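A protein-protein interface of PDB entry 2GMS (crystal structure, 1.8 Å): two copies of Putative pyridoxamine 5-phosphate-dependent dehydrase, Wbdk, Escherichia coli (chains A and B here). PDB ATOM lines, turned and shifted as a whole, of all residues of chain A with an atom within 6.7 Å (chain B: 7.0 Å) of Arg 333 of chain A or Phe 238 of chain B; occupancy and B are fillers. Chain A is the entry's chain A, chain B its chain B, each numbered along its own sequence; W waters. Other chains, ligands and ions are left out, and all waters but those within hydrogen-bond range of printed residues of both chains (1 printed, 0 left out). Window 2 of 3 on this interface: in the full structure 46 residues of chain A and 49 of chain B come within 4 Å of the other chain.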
ATOM      1  N   LEU A   8      17.430  -9.978 -22.622  1.00  0.00           N
ATOM      2  CA  LEU A   8      18.304 -11.066 -22.286  1.00  0.00           C
ATOM      3  C   LEU A   8      17.983 -12.220 -23.201  1.00  0.00           C
ATOM      4  O   LEU A   8      18.891 -12.902 -23.665  1.00  0.00           O
ATOM      5  CB  LEU A   8      18.118 -11.511 -20.827  1.00  0.00           C
ATOM      6  CG  LEU A   8      18.810 -10.597 -19.828  1.00  0.00           C
ATOM      7  CD1 LEU A   8      18.262 -10.870 -18.438  1.00  0.00           C
ATOM      8  CD2 LEU A   8      20.314 -10.831 -19.873  1.00  0.00           C
ATOM      9  N   TRP A  90      24.505 -23.579 -11.957  1.00  0.00           N
ATOM     10  CA  TRP A  90      23.078 -23.508 -11.701  1.00  0.00           C
ATOM     11  C   TRP A  90      22.751 -24.395 -10.491  1.00  0.00           C
ATOM     12  O   TRP A  90      23.463 -25.341 -10.190  1.00  0.00           O
ATOM     13  CB  TRP A  90      22.273 -23.894 -12.960  1.00  0.00           C
ATOM     14  CG  TRP A  90      20.800 -23.772 -12.734  1.00  0.00           C
ATOM     15  CD1 TRP A  90      19.899 -24.780 -12.651  1.00  0.00           C
ATOM     16  CD2 TRP A  90      20.089 -22.565 -12.500  1.00  0.00           C
ATOM     17  NE1 TRP A  90      18.660 -24.268 -12.377  1.00  0.00           N
ATOM     18  CE2 TRP A  90      18.742 -22.910 -12.275  1.00  0.00           C
ATOM     19  CE3 TRP A  90      20.476 -21.223 -12.442  1.00  0.00           C
ATOM     20  CZ2 TRP A  90      17.764 -21.950 -12.000  1.00  0.00           C
ATOM     21  CZ3 TRP A  90      19.508 -20.272 -12.177  1.00  0.00           C
ATOM     22  CH2 TRP A  90      18.167 -20.625 -11.969  1.00  0.00           C
ATOM     23  N   GLU A 164      24.857 -24.805 -20.718  1.00  0.00           N
ATOM     24  CA  GLU A 164      25.027 -23.441 -21.235  1.00  0.00           C
ATOM     25  C   GLU A 164      25.965 -23.350 -22.428  1.00  0.00           C
ATOM     26  O   GLU A 164      26.127 -22.273 -23.014  1.00  0.00           O
ATOM     27  CB  GLU A 164      25.619 -22.494 -20.172  1.00  0.00           C
ATOM     28  CG  GLU A 164      24.665 -22.308 -18.964  1.00  0.00           C
ATOM     29  CD  GLU A 164      25.291 -21.533 -17.825  1.00  0.00           C
ATOM     30  OE1 GLU A 164      26.410 -21.044 -17.885  1.00  0.00           O
ATOM     31  OE2 GLU A 164      24.516 -21.457 -16.766  1.00  0.00           O
ATOM     32  N   PHE A 304      26.990 -18.025 -24.728  1.00  0.00           N
ATOM     33  CA  PHE A 304      25.635 -18.062 -24.270  1.00  0.00           C
ATOM     34  C   PHE A 304      25.190 -16.646 -23.962  1.00  0.00           C
ATOM     35  O   PHE A 304      24.084 -16.232 -24.270  1.00  0.00           O
ATOM     36  CB  PHE A 304      25.630 -18.906 -22.996  1.00  0.00           C
ATOM     37  CG  PHE A 304      24.261 -19.062 -22.405  1.00  0.00           C
ATOM     38  CD1 PHE A 304      23.382 -20.003 -22.932  1.00  0.00           C
ATOM     39  CD2 PHE A 304      23.839 -18.286 -21.328  1.00  0.00           C
ATOM     40  CE1 PHE A 304      22.114 -20.183 -22.386  1.00  0.00           C
ATOM     41  CE2 PHE A 304      22.562 -18.435 -20.787  1.00  0.00           C
ATOM     42  CZ  PHE A 304      21.706 -19.399 -21.312  1.00  0.00           C
ATOM     43  N   ARG A 318      28.558  -2.084  -8.416  1.00  0.00           N
ATOM     44  CA  ARG A 318      27.657  -2.847  -9.245  1.00  0.00           C
ATOM     45  C   ARG A 318      26.249  -2.314  -9.257  1.00  0.00           C
ATOM     46  O   ARG A 318      25.668  -2.182 -10.326  1.00  0.00           O
ATOM     47  CB  ARG A 318      27.623  -4.339  -8.968  1.00  0.00           C
ATOM     48  CG  ARG A 318      26.656  -5.018  -9.940  1.00  0.00           C
ATOM     49  CD  ARG A 318      26.542  -6.522  -9.754  1.00  0.00           C
ATOM     50  NE  ARG A 318      26.003  -6.876  -8.446  1.00  0.00           N
ATOM     51  CZ  ARG A 318      26.144  -8.078  -7.911  1.00  0.00           C
ATOM     52  NH1 ARG A 318      26.781  -9.064  -8.560  1.00  0.00           N
ATOM     53  NH2 ARG A 318      25.630  -8.292  -6.700  1.00  0.00           N
ATOM     54  N   VAL A 322      23.839  -1.562 -12.587  1.00  0.00           N
ATOM     55  CA  VAL A 322      22.573  -2.202 -12.841  1.00  0.00           C
ATOM     56  C   VAL A 322      21.477  -1.171 -13.063  1.00  0.00           C
ATOM     57  O   VAL A 322      20.712  -1.214 -14.035  1.00  0.00           O
ATOM     58  CB  VAL A 322      22.244  -3.176 -11.741  1.00  0.00           C
ATOM     59  CG1 VAL A 322      20.831  -3.672 -11.999  1.00  0.00           C
ATOM     60  CG2 VAL A 322      23.212  -4.344 -11.837  1.00  0.00           C
ATOM     61  N   ASN A 326      19.322  -0.642 -16.481  1.00  0.00           N
ATOM     62  CA  ASN A 326      17.883  -0.708 -16.421  1.00  0.00           C
ATOM     63  C   ASN A 326      17.150   0.509 -16.955  1.00  0.00           C
ATOM     64  O   ASN A 326      16.171   0.397 -17.697  1.00  0.00           O
ATOM     65  CB  ASN A 326      17.392  -1.236 -15.050  1.00  0.00           C
ATOM     66  CG  ASN A 326      17.635  -2.737 -14.882  1.00  0.00           C
ATOM     67  OD1 ASN A 326      17.890  -3.210 -13.759  1.00  0.00           O
ATOM     68  ND2 ASN A 326      17.579  -3.495 -15.996  1.00  0.00           N
ATOM     69  N   GLU A 331      18.368  -5.236 -20.207  1.00  0.00           N
ATOM     70  CA  GLU A 331      18.215  -6.313 -19.223  1.00  0.00           C
ATOM     71  C   GLU A 331      19.579  -6.889 -18.828  1.00  0.00           C
ATOM     72  O   GLU A 331      20.466  -7.130 -19.662  1.00  0.00           O
ATOM     73  CB  GLU A 331      17.356  -7.442 -19.800  1.00  0.00           C
ATOM     74  CG  GLU A 331      15.880  -7.088 -19.777  1.00  0.00           C
ATOM     75  CD  GLU A 331      14.964  -8.218 -20.167  1.00  0.00           C
ATOM     76  OE1 GLU A 331      15.266  -8.994 -21.134  1.00  0.00           O
ATOM     77  OE2 GLU A 331      13.883  -8.355 -19.496  1.00  0.00           O
ATOM     78  N   CYS A 332      19.742  -7.097 -17.544  1.00  0.00           N
ATOM     79  CA  CYS A 332      20.976  -7.677 -17.021  1.00  0.00           C
ATOM     80  C   CYS A 332      20.588  -8.634 -15.892  1.00  0.00           C
ATOM     81  O   CYS A 332      19.509  -8.525 -15.298  1.00  0.00           O
ATOM     82  CB  CYS A 332      21.964  -6.603 -16.580  1.00  0.00           C
ATOM     83  SG  CYS A 332      21.345  -5.522 -15.242  1.00  0.00           S
ATOM     84  N   ARG A 333      21.492  -9.571 -15.642  1.00  0.00           N
ATOM     85  CA  ARG A 333      21.274 -10.741 -14.665  1.00  0.00           C
ATOM     86  C   ARG A 333      22.649 -10.854 -13.882  1.00  0.00           C
ATOM     87  O   ARG A 333      23.712 -10.328 -14.307  1.00  0.00           O
ATOM     88  CB  ARG A 333      20.761 -12.063 -15.481  1.00  0.00           C
ATOM     89  CG  ARG A 333      21.411 -13.387 -15.070  1.00  0.00           C
ATOM     90  CD  ARG A 333      21.041 -14.570 -15.976  1.00  0.00           C
ATOM     91  NE  ARG A 333      21.024 -15.827 -15.232  1.00  0.00           N
ATOM     92  CZ  ARG A 333      20.444 -16.950 -15.646  1.00  0.00           C
ATOM     93  NH1 ARG A 333      19.534 -16.931 -16.635  1.00  0.00           N
ATOM     94  NH2 ARG A 333      20.733 -18.138 -15.116  1.00  0.00           N
ATOM     95  N   PRO A 334      22.644 -11.512 -12.765  1.00  0.00           N
ATOM     96  CA  PRO A 334      23.876 -11.905 -12.156  1.00  0.00           C
ATOM     97  C   PRO A 334      24.452 -12.998 -13.030  1.00  0.00           C
ATOM     98  O   PRO A 334      23.798 -13.552 -13.915  1.00  0.00           O
ATOM     99  CB  PRO A 334      23.529 -12.521 -10.797  1.00  0.00           C
ATOM    100  CG  PRO A 334      22.024 -12.396 -10.610  1.00  0.00           C
ATOM    101  CD  PRO A 334      21.512 -11.625 -11.810  1.00  0.00           C
ATOM    102  N   ILE A 335      25.707 -13.295 -12.789  1.00  0.00           N
ATOM    103  CA  ILE A 335      26.308 -14.353 -13.541  1.00  0.00           C
ATOM    104  C   ILE A 335      25.815 -15.649 -12.916  1.00  0.00           C
ATOM    105  O   ILE A 335      26.216 -16.085 -11.825  1.00  0.00           O
ATOM    106  CB  ILE A 335      27.815 -14.265 -13.545  1.00  0.00           C
ATOM    107  CG1 ILE A 335      28.244 -12.986 -14.252  1.00  0.00           C
ATOM    108  CG2 ILE A 335      28.415 -15.510 -14.214  1.00  0.00           C
ATOM    109  CD1 ILE A 335      29.702 -12.593 -13.957  1.00  0.00           C
ATOM    110  N   VAL A 336      24.881 -16.248 -13.643  1.00  0.00           N
ATOM    111  CA  VAL A 336      24.262 -17.482 -13.221  1.00  0.00           C
ATOM    112  C   VAL A 336      23.695 -17.225 -11.824  1.00  0.00           C
ATOM    113  O   VAL A 336      22.899 -16.316 -11.617  1.00  0.00           O
ATOM    114  CB  VAL A 336      25.207 -18.706 -13.392  1.00  0.00           C
ATOM    115  CG1 VAL A 336      24.497 -20.049 -13.276  1.00  0.00           C
ATOM    116  CG2 VAL A 336      25.917 -18.690 -14.732  1.00  0.00           C
ATOM    117  N   THR A 337      24.151 -17.980 -10.860  1.00  0.00           N
ATOM    118  CA  THR A 337      23.702 -17.865  -9.502  1.00  0.00           C
ATOM    119  C   THR A 337      24.672 -17.071  -8.648  1.00  0.00           C
ATOM    120  O   THR A 337      24.364 -16.815  -7.486  1.00  0.00           O
ATOM    121  CB  THR A 337      23.711 -19.278  -8.871  1.00  0.00           C
ATOM    122  OG1 THR A 337      25.050 -19.801  -8.757  1.00  0.00           O
ATOM    123  CG2 THR A 337      22.820 -20.208  -9.678  1.00  0.00           C
ATOM    124  N   LYS A 342      26.947 -19.070  -1.045  1.00  0.00           N
ATOM    125  CA  LYS A 342      26.254 -18.105  -0.239  1.00  0.00           C
ATOM    126  C   LYS A 342      24.869 -18.634   0.193  1.00  0.00           C
ATOM    127  O   LYS A 342      24.200 -18.080   1.069  1.00  0.00           O
ATOM    128  CB  LYS A 342      26.081 -16.820  -1.019  1.00  0.00           C
ATOM    129  CG  LYS A 342      24.935 -16.929  -2.025  1.00  0.00           C
ATOM    130  CD  LYS A 342      24.891 -15.795  -3.045  1.00  0.00           C
ATOM    131  CE  LYS A 342      24.199 -16.202  -4.342  1.00  0.00           C
ATOM    132  NZ  LYS A 342      23.493 -15.100  -5.018  1.00  0.00           N
ATOM    133  N   ASP A 365      30.542 -12.741  -7.229  1.00  0.00           N
ATOM    134  CA  ASP A 365      29.226 -12.606  -6.621  1.00  0.00           C
ATOM    135  C   ASP A 365      28.796 -11.175  -6.384  1.00  0.00           C
ATOM    136  O   ASP A 365      27.634 -10.780  -6.525  1.00  0.00           O
ATOM    137  CB  ASP A 365      29.125 -13.349  -5.277  1.00  0.00           C
ATOM    138  CG  ASP A 365      27.686 -13.590  -4.901  1.00  0.00           C
ATOM    139  OD1 ASP A 365      27.022 -14.484  -5.370  1.00  0.00           O
ATOM    140  OD2 ASP A 365      27.211 -12.729  -4.053  1.00  0.00           O
ATOM    141  N   GLY A 368      29.993  -9.164 -10.408  1.00  0.00           N
ATOM    142  CA  GLY A 368      29.702  -9.597 -11.763  1.00  0.00           C
ATOM    143  C   GLY A 368      28.258  -9.338 -12.221  1.00  0.00           C
ATOM    144  O   GLY A 368      27.326  -9.180 -11.418  1.00  0.00           O
ATOM    145  N   LEU A 369      28.112  -9.303 -13.545  1.00  0.00           N
ATOM    146  CA  LEU A 369      26.840  -9.136 -14.216  1.00  0.00           C
ATOM    147  C   LEU A 369      26.917  -9.681 -15.623  1.00  0.00           C
ATOM    148  O   LEU A 369      28.012  -9.845 -16.149  1.00  0.00           O
ATOM    149  CB  LEU A 369      26.103  -7.792 -14.068  1.00  0.00           C
ATOM    150  CG  LEU A 369      26.951  -6.570 -14.378  1.00  0.00           C
ATOM    151  CD1 LEU A 369      27.986  -6.886 -15.444  1.00  0.00           C
ATOM    152  CD2 LEU A 369      26.027  -5.467 -14.869  1.00  0.00           C
ATOM    153  N   PHE A 370      25.756  -9.944 -16.206  1.00  0.00           N
ATOM    154  CA  PHE A 370      25.630 -10.544 -17.510  1.00  0.00           C
ATOM    155  C   PHE A 370      24.483  -9.918 -18.316  1.00  0.00           C
ATOM    156  O   PHE A 370      23.422  -9.594 -17.745  1.00  0.00           O
ATOM    157  CB  PHE A 370      25.302 -12.028 -17.156  1.00  0.00           C
ATOM    158  CG  PHE A 370      24.744 -12.949 -18.201  1.00  0.00           C
ATOM    159  CD1 PHE A 370      25.578 -13.835 -18.879  1.00  0.00           C
ATOM    160  CD2 PHE A 370      23.381 -12.964 -18.496  1.00  0.00           C
ATOM    161  CE1 PHE A 370      25.069 -14.707 -19.841  1.00  0.00           C
ATOM    162  CE2 PHE A 370      22.854 -13.833 -19.450  1.00  0.00           C
ATOM    163  CZ  PHE A 370      23.705 -14.705 -20.125  1.00  0.00           C
ATOM    164  N   VAL A 371      24.719  -9.739 -19.640  1.00  0.00           N
ATOM    165  CA  VAL A 371      23.744  -9.261 -20.633  1.00  0.00           C
ATOM    166  C   VAL A 371      23.657 -10.352 -21.693  1.00  0.00           C
ATOM    167  O   VAL A 371      24.567 -11.191 -21.801  1.00  0.00           O
ATOM    168  CB  VAL A 371      23.992  -7.883 -21.233  1.00  0.00           C
ATOM    169  CG1 VAL A 371      23.940  -6.832 -20.124  1.00  0.00           C
ATOM    170  CG2 VAL A 371      25.340  -7.869 -21.948  1.00  0.00           C
ATOM    171  N   ARG B 221      11.181 -17.886  -6.521  1.00  0.00           N
ATOM    172  CA  ARG B 221      10.375 -17.184  -7.508  1.00  0.00           C
ATOM    173  C   ARG B 221       8.880 -17.446  -7.509  1.00  0.00           C
ATOM    174  O   ARG B 221       8.090 -16.570  -7.862  1.00  0.00           O
ATOM    175  CB  ARG B 221      10.858 -17.350  -8.920  1.00  0.00           C
ATOM    176  CG  ARG B 221      12.217 -16.731  -9.067  1.00  0.00           C
ATOM    177  CD  ARG B 221      12.577 -16.579 -10.530  1.00  0.00           C
ATOM    178  NE  ARG B 221      14.018 -16.538 -10.645  1.00  0.00           N
ATOM    179  CZ  ARG B 221      14.685 -16.670 -11.779  1.00  0.00           C
ATOM    180  NH1 ARG B 221      14.076 -16.849 -12.942  1.00  0.00           N
ATOM    181  NH2 ARG B 221      16.017 -16.616 -11.740  1.00  0.00           N
ATOM    182  N   ASP B 235      13.269  -7.581  -1.315  1.00  0.00           N
ATOM    183  CA  ASP B 235      12.776  -6.834  -2.447  1.00  0.00           C
ATOM    184  C   ASP B 235      13.817  -6.652  -3.549  1.00  0.00           C
ATOM    185  O   ASP B 235      13.533  -6.163  -4.638  1.00  0.00           O
ATOM    186  CB  ASP B 235      12.088  -5.541  -2.000  1.00  0.00           C
ATOM    187  CG  ASP B 235      10.828  -5.862  -1.233  1.00  0.00           C
ATOM    188  OD1 ASP B 235       9.851  -6.352  -1.783  1.00  0.00           O
ATOM    189  OD2 ASP B 235      10.930  -5.581   0.053  1.00  0.00           O
ATOM    190  N   ASP B 236      15.041  -7.073  -3.270  1.00  0.00           N
ATOM    191  CA  ASP B 236      16.112  -6.992  -4.240  1.00  0.00           C
ATOM    192  C   ASP B 236      16.067  -8.218  -5.140  1.00  0.00           C
ATOM    193  O   ASP B 236      16.540  -9.296  -4.753  1.00  0.00           O
ATOM    194  CB  ASP B 236      17.479  -6.917  -3.527  1.00  0.00           C
ATOM    195  CG  ASP B 236      18.610  -6.523  -4.443  1.00  0.00           C
ATOM    196  OD1 ASP B 236      18.448  -6.229  -5.619  1.00  0.00           O
ATOM    197  OD2 ASP B 236      19.779  -6.523  -3.838  1.00  0.00           O
ATOM    198  N   GLN B 237      15.484  -8.064  -6.339  1.00  0.00           N
ATOM    199  CA  GLN B 237      15.379  -9.194  -7.257  1.00  0.00           C
ATOM    200  C   GLN B 237      16.689  -9.723  -7.759  1.00  0.00           C
ATOM    201  O   GLN B 237      16.793 -10.906  -8.092  1.00  0.00           O
ATOM    202  CB  GLN B 237      14.330  -9.125  -8.376  1.00  0.00           C
ATOM    203  CG  GLN B 237      13.698  -7.750  -8.617  1.00  0.00           C
ATOM    204  CD  GLN B 237      12.397  -7.864  -9.401  1.00  0.00           C
ATOM    205  OE1 GLN B 237      12.357  -7.671 -10.639  1.00  0.00           O
ATOM    206  NE2 GLN B 237      11.313  -8.155  -8.671  1.00  0.00           N
ATOM    207  N   PHE B 238      17.665  -8.826  -7.801  1.00  0.00           N
ATOM    208  CA  PHE B 238      18.987  -9.219  -8.208  1.00  0.00           C
ATOM    209  C   PHE B 238      19.438 -10.296  -7.239  1.00  0.00           C
ATOM    210  O   PHE B 238      20.129 -11.251  -7.596  1.00  0.00           O
ATOM    211  CB  PHE B 238      19.967  -8.028  -8.219  1.00  0.00           C
ATOM    212  CG  PHE B 238      21.013  -8.154  -9.306  1.00  0.00           C
ATOM    213  CD1 PHE B 238      20.704  -7.913 -10.647  1.00  0.00           C
ATOM    214  CD2 PHE B 238      22.320  -8.532  -8.997  1.00  0.00           C
ATOM    215  CE1 PHE B 238      21.667  -8.032 -11.654  1.00  0.00           C
ATOM    216  CE2 PHE B 238      23.295  -8.657  -9.992  1.00  0.00           C
ATOM    217  CZ  PHE B 238      22.973  -8.399 -11.326  1.00  0.00           C
ATOM    218  N   GLU B 239      18.990 -10.131  -5.992  1.00  0.00           N
ATOM    219  CA  GLU B 239      19.322 -11.071  -4.938  1.00  0.00           C
ATOM    220  C   GLU B 239      18.289 -12.157  -4.806  1.00  0.00           C
ATOM    221  O   GLU B 239      18.569 -13.351  -4.923  1.00  0.00           O
ATOM    222  CB  GLU B 239      19.409 -10.345  -3.585  1.00  0.00           C
ATOM    223  CG  GLU B 239      20.719  -9.549  -3.444  1.00  0.00           C
ATOM    224  CD  GLU B 239      21.914 -10.301  -3.977  1.00  0.00           C
ATOM    225  OE1 GLU B 239      22.177 -11.453  -3.675  1.00  0.00           O
ATOM    226  OE2 GLU B 239      22.656  -9.553  -4.777  1.00  0.00           O
ATOM    227  N   GLU B 240      17.092 -11.667  -4.523  1.00  0.00           N
ATOM    228  CA  GLU B 240      15.942 -12.498  -4.294  1.00  0.00           C
ATOM    229  C   GLU B 240      15.697 -13.551  -5.353  1.00  0.00           C
ATOM    230  O   GLU B 240      15.489 -14.708  -5.028  1.00  0.00           O
ATOM    231  CB  GLU B 240      14.658 -11.716  -3.937  1.00  0.00           C
ATOM    232  CG  GLU B 240      13.552 -12.680  -3.465  1.00  0.00           C
ATOM    233  CD  GLU B 240      13.935 -13.360  -2.170  1.00  0.00           C
ATOM    234  OE1 GLU B 240      14.598 -12.814  -1.317  1.00  0.00           O
ATOM    235  OE2 GLU B 240      13.460 -14.577  -2.044  1.00  0.00           O
ATOM    236  N   SER B 241      15.722 -13.147  -6.606  1.00  0.00           N
ATOM    237  CA  SER B 241      15.479 -14.052  -7.714  1.00  0.00           C
ATOM    238  C   SER B 241      16.529 -15.144  -7.888  1.00  0.00           C
ATOM    239  O   SER B 241      16.364 -16.097  -8.686  1.00  0.00           O
ATOM    240  CB  SER B 241      15.337 -13.270  -9.006  1.00  0.00           C
ATOM    241  OG  SER B 241      14.023 -12.793  -9.145  1.00  0.00           O
ATOM    242  N   PHE B 242      17.645 -14.975  -7.185  1.00  0.00           N
ATOM    243  CA  PHE B 242      18.722 -15.924  -7.318  1.00  0.00           C
ATOM    244  C   PHE B 242      19.048 -16.726  -6.076  1.00  0.00           C
ATOM    245  O   PHE B 242      20.148 -17.242  -5.927  1.00  0.00           O
ATOM    246  CB  PHE B 242      19.927 -15.238  -7.987  1.00  0.00           C
ATOM    247  CG  PHE B 242      19.516 -14.856  -9.393  1.00  0.00           C
ATOM    248  CD1 PHE B 242      18.852 -13.654  -9.655  1.00  0.00           C
ATOM    249  CD2 PHE B 242      19.711 -15.745 -10.454  1.00  0.00           C
ATOM    250  CE1 PHE B 242      18.434 -13.317 -10.946  1.00  0.00           C
ATOM    251  CE2 PHE B 242      19.301 -15.429 -11.752  1.00  0.00           C
ATOM    252  CZ  PHE B 242      18.657 -14.214 -11.994  1.00  0.00           C
ATOM    253  N   LYS B 243      18.079 -16.834  -5.187  1.00  0.00           N
ATOM    254  CA  LYS B 243      18.360 -17.593  -4.012  1.00  0.00           C
ATOM    255  C   LYS B 243      17.753 -18.980  -4.024  1.00  0.00           C
ATOM    256  O   LYS B 243      16.631 -19.187  -4.485  1.00  0.00           O
ATOM    257  CB  LYS B 243      18.247 -16.842  -2.705  1.00  0.00           C
ATOM    258  CG  LYS B 243      16.850 -16.643  -2.186  1.00  0.00           C
ATOM    259  CD  LYS B 243      16.860 -15.710  -0.985  1.00  0.00           C
ATOM    260  CE  LYS B 243      17.721 -14.472  -1.222  1.00  0.00           C
ATOM    261  NZ  LYS B 243      17.184 -13.237  -0.642  1.00  0.00           N
HETATM  262  O   HOH W   1      22.574 -13.353  -7.123  1.00  0.00           O
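Water W1 bridges NZ of Lys 342 of chain A and O of Phe 238 of chain B.
No position is printed for both chains. Of the 7 pairs that touch across the chains among the printed residues, none has its exchanged pair printed and touching as well.
Printed residues of chain A that touch a printed residue of chain B: Arg 318, Arg 333, Pro 334 and Val 336. Hydrophobic or aromatic side chains of chain A that line the printed part of chain B: Pro 334. Of the 10 printed residues of chain B, 3 touch a printed residue of chain A. Among the printed residues, 7 pairs touch across the chains. Among the printed residues, Asp or Glu carboxylates within 4 Å of a Lys or Arg side-chain nitrogen of the other chain: Arg 318 of chain A with Glu 239 of chain B (3.8 Å).
Of chain B, only Phe 238 and Phe 242 come within 4 Å of Arg 333 of chain A. Of the printed residues of chain B, Pro 334 of chain A touches Phe 238 and Phe 242. Printed residues of chain B within 4 Å of Val 336 of chain A: Phe 242 (3.4 Å). Of the printed residues of chain A, Phe 238 of chain B touches Arg 318 (3.6 Å), Arg 333 (3.6 Å) and Pro 334 (3.4 Å). Of the printed residues of chain A, Glu 239 of chain B touches Arg 318. Printed residues of chain A within 4 Å of Phe 242 of chain B: Arg 333 (3.9 Å), Pro 334 (3.5 Å) and Val 336 (3.4 Å). Lys 243 of chain B touches none of the printed residues of chain A. The nearest residue of chain B that does not touch Arg 333 of chain A is Arg 221 of chain B (5.9 Å). The nearest printed residue of chain A that does not touch Phe 238 of chain B is Val 322 of chain A (4.003 Å).
The side-chain carboxylate (OE2) of Glu 239 of chain B lies within salt-bridge range of the guanidinium group (NH2) of Arg 318 of chain A.
Arg 318 of chain A touches Phe 238 of chain B (CZ to CE2, 3.6 Å). Arg 333 of chain A touches Phe 238 of chain B (C to CZ, 3.6 Å). Arg 333 of chain A touches Phe 242 of chain B (NE to CE2, 3.9 Å). Pro 334 of chain A touches Phe 238 of chain B (N to CZ, 3.4 Å). Pro 334 of chain A touches Phe 242 of chain B. Val 336 of chain A touches Phe 242 of chain B (O to CD2, 3.4 Å).
NH1 of Arg 318 of chain A sits at hydrogen-bond distance from O of Gly 368 of chain A, at 2.9 Å. OD1 of Asp 236 of chain B sits close to N of Phe 238 of chain B. O of Arg 333 of chain A is in hydrogen-bond range of N of Phe 370 of chain A (2.8 Å). The guanidinium group of Arg 318 of chain A lies within hydrogen-bond range of the backbone carbonyl oxygen of Asp 365 of chain A, 2.8 Å away.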
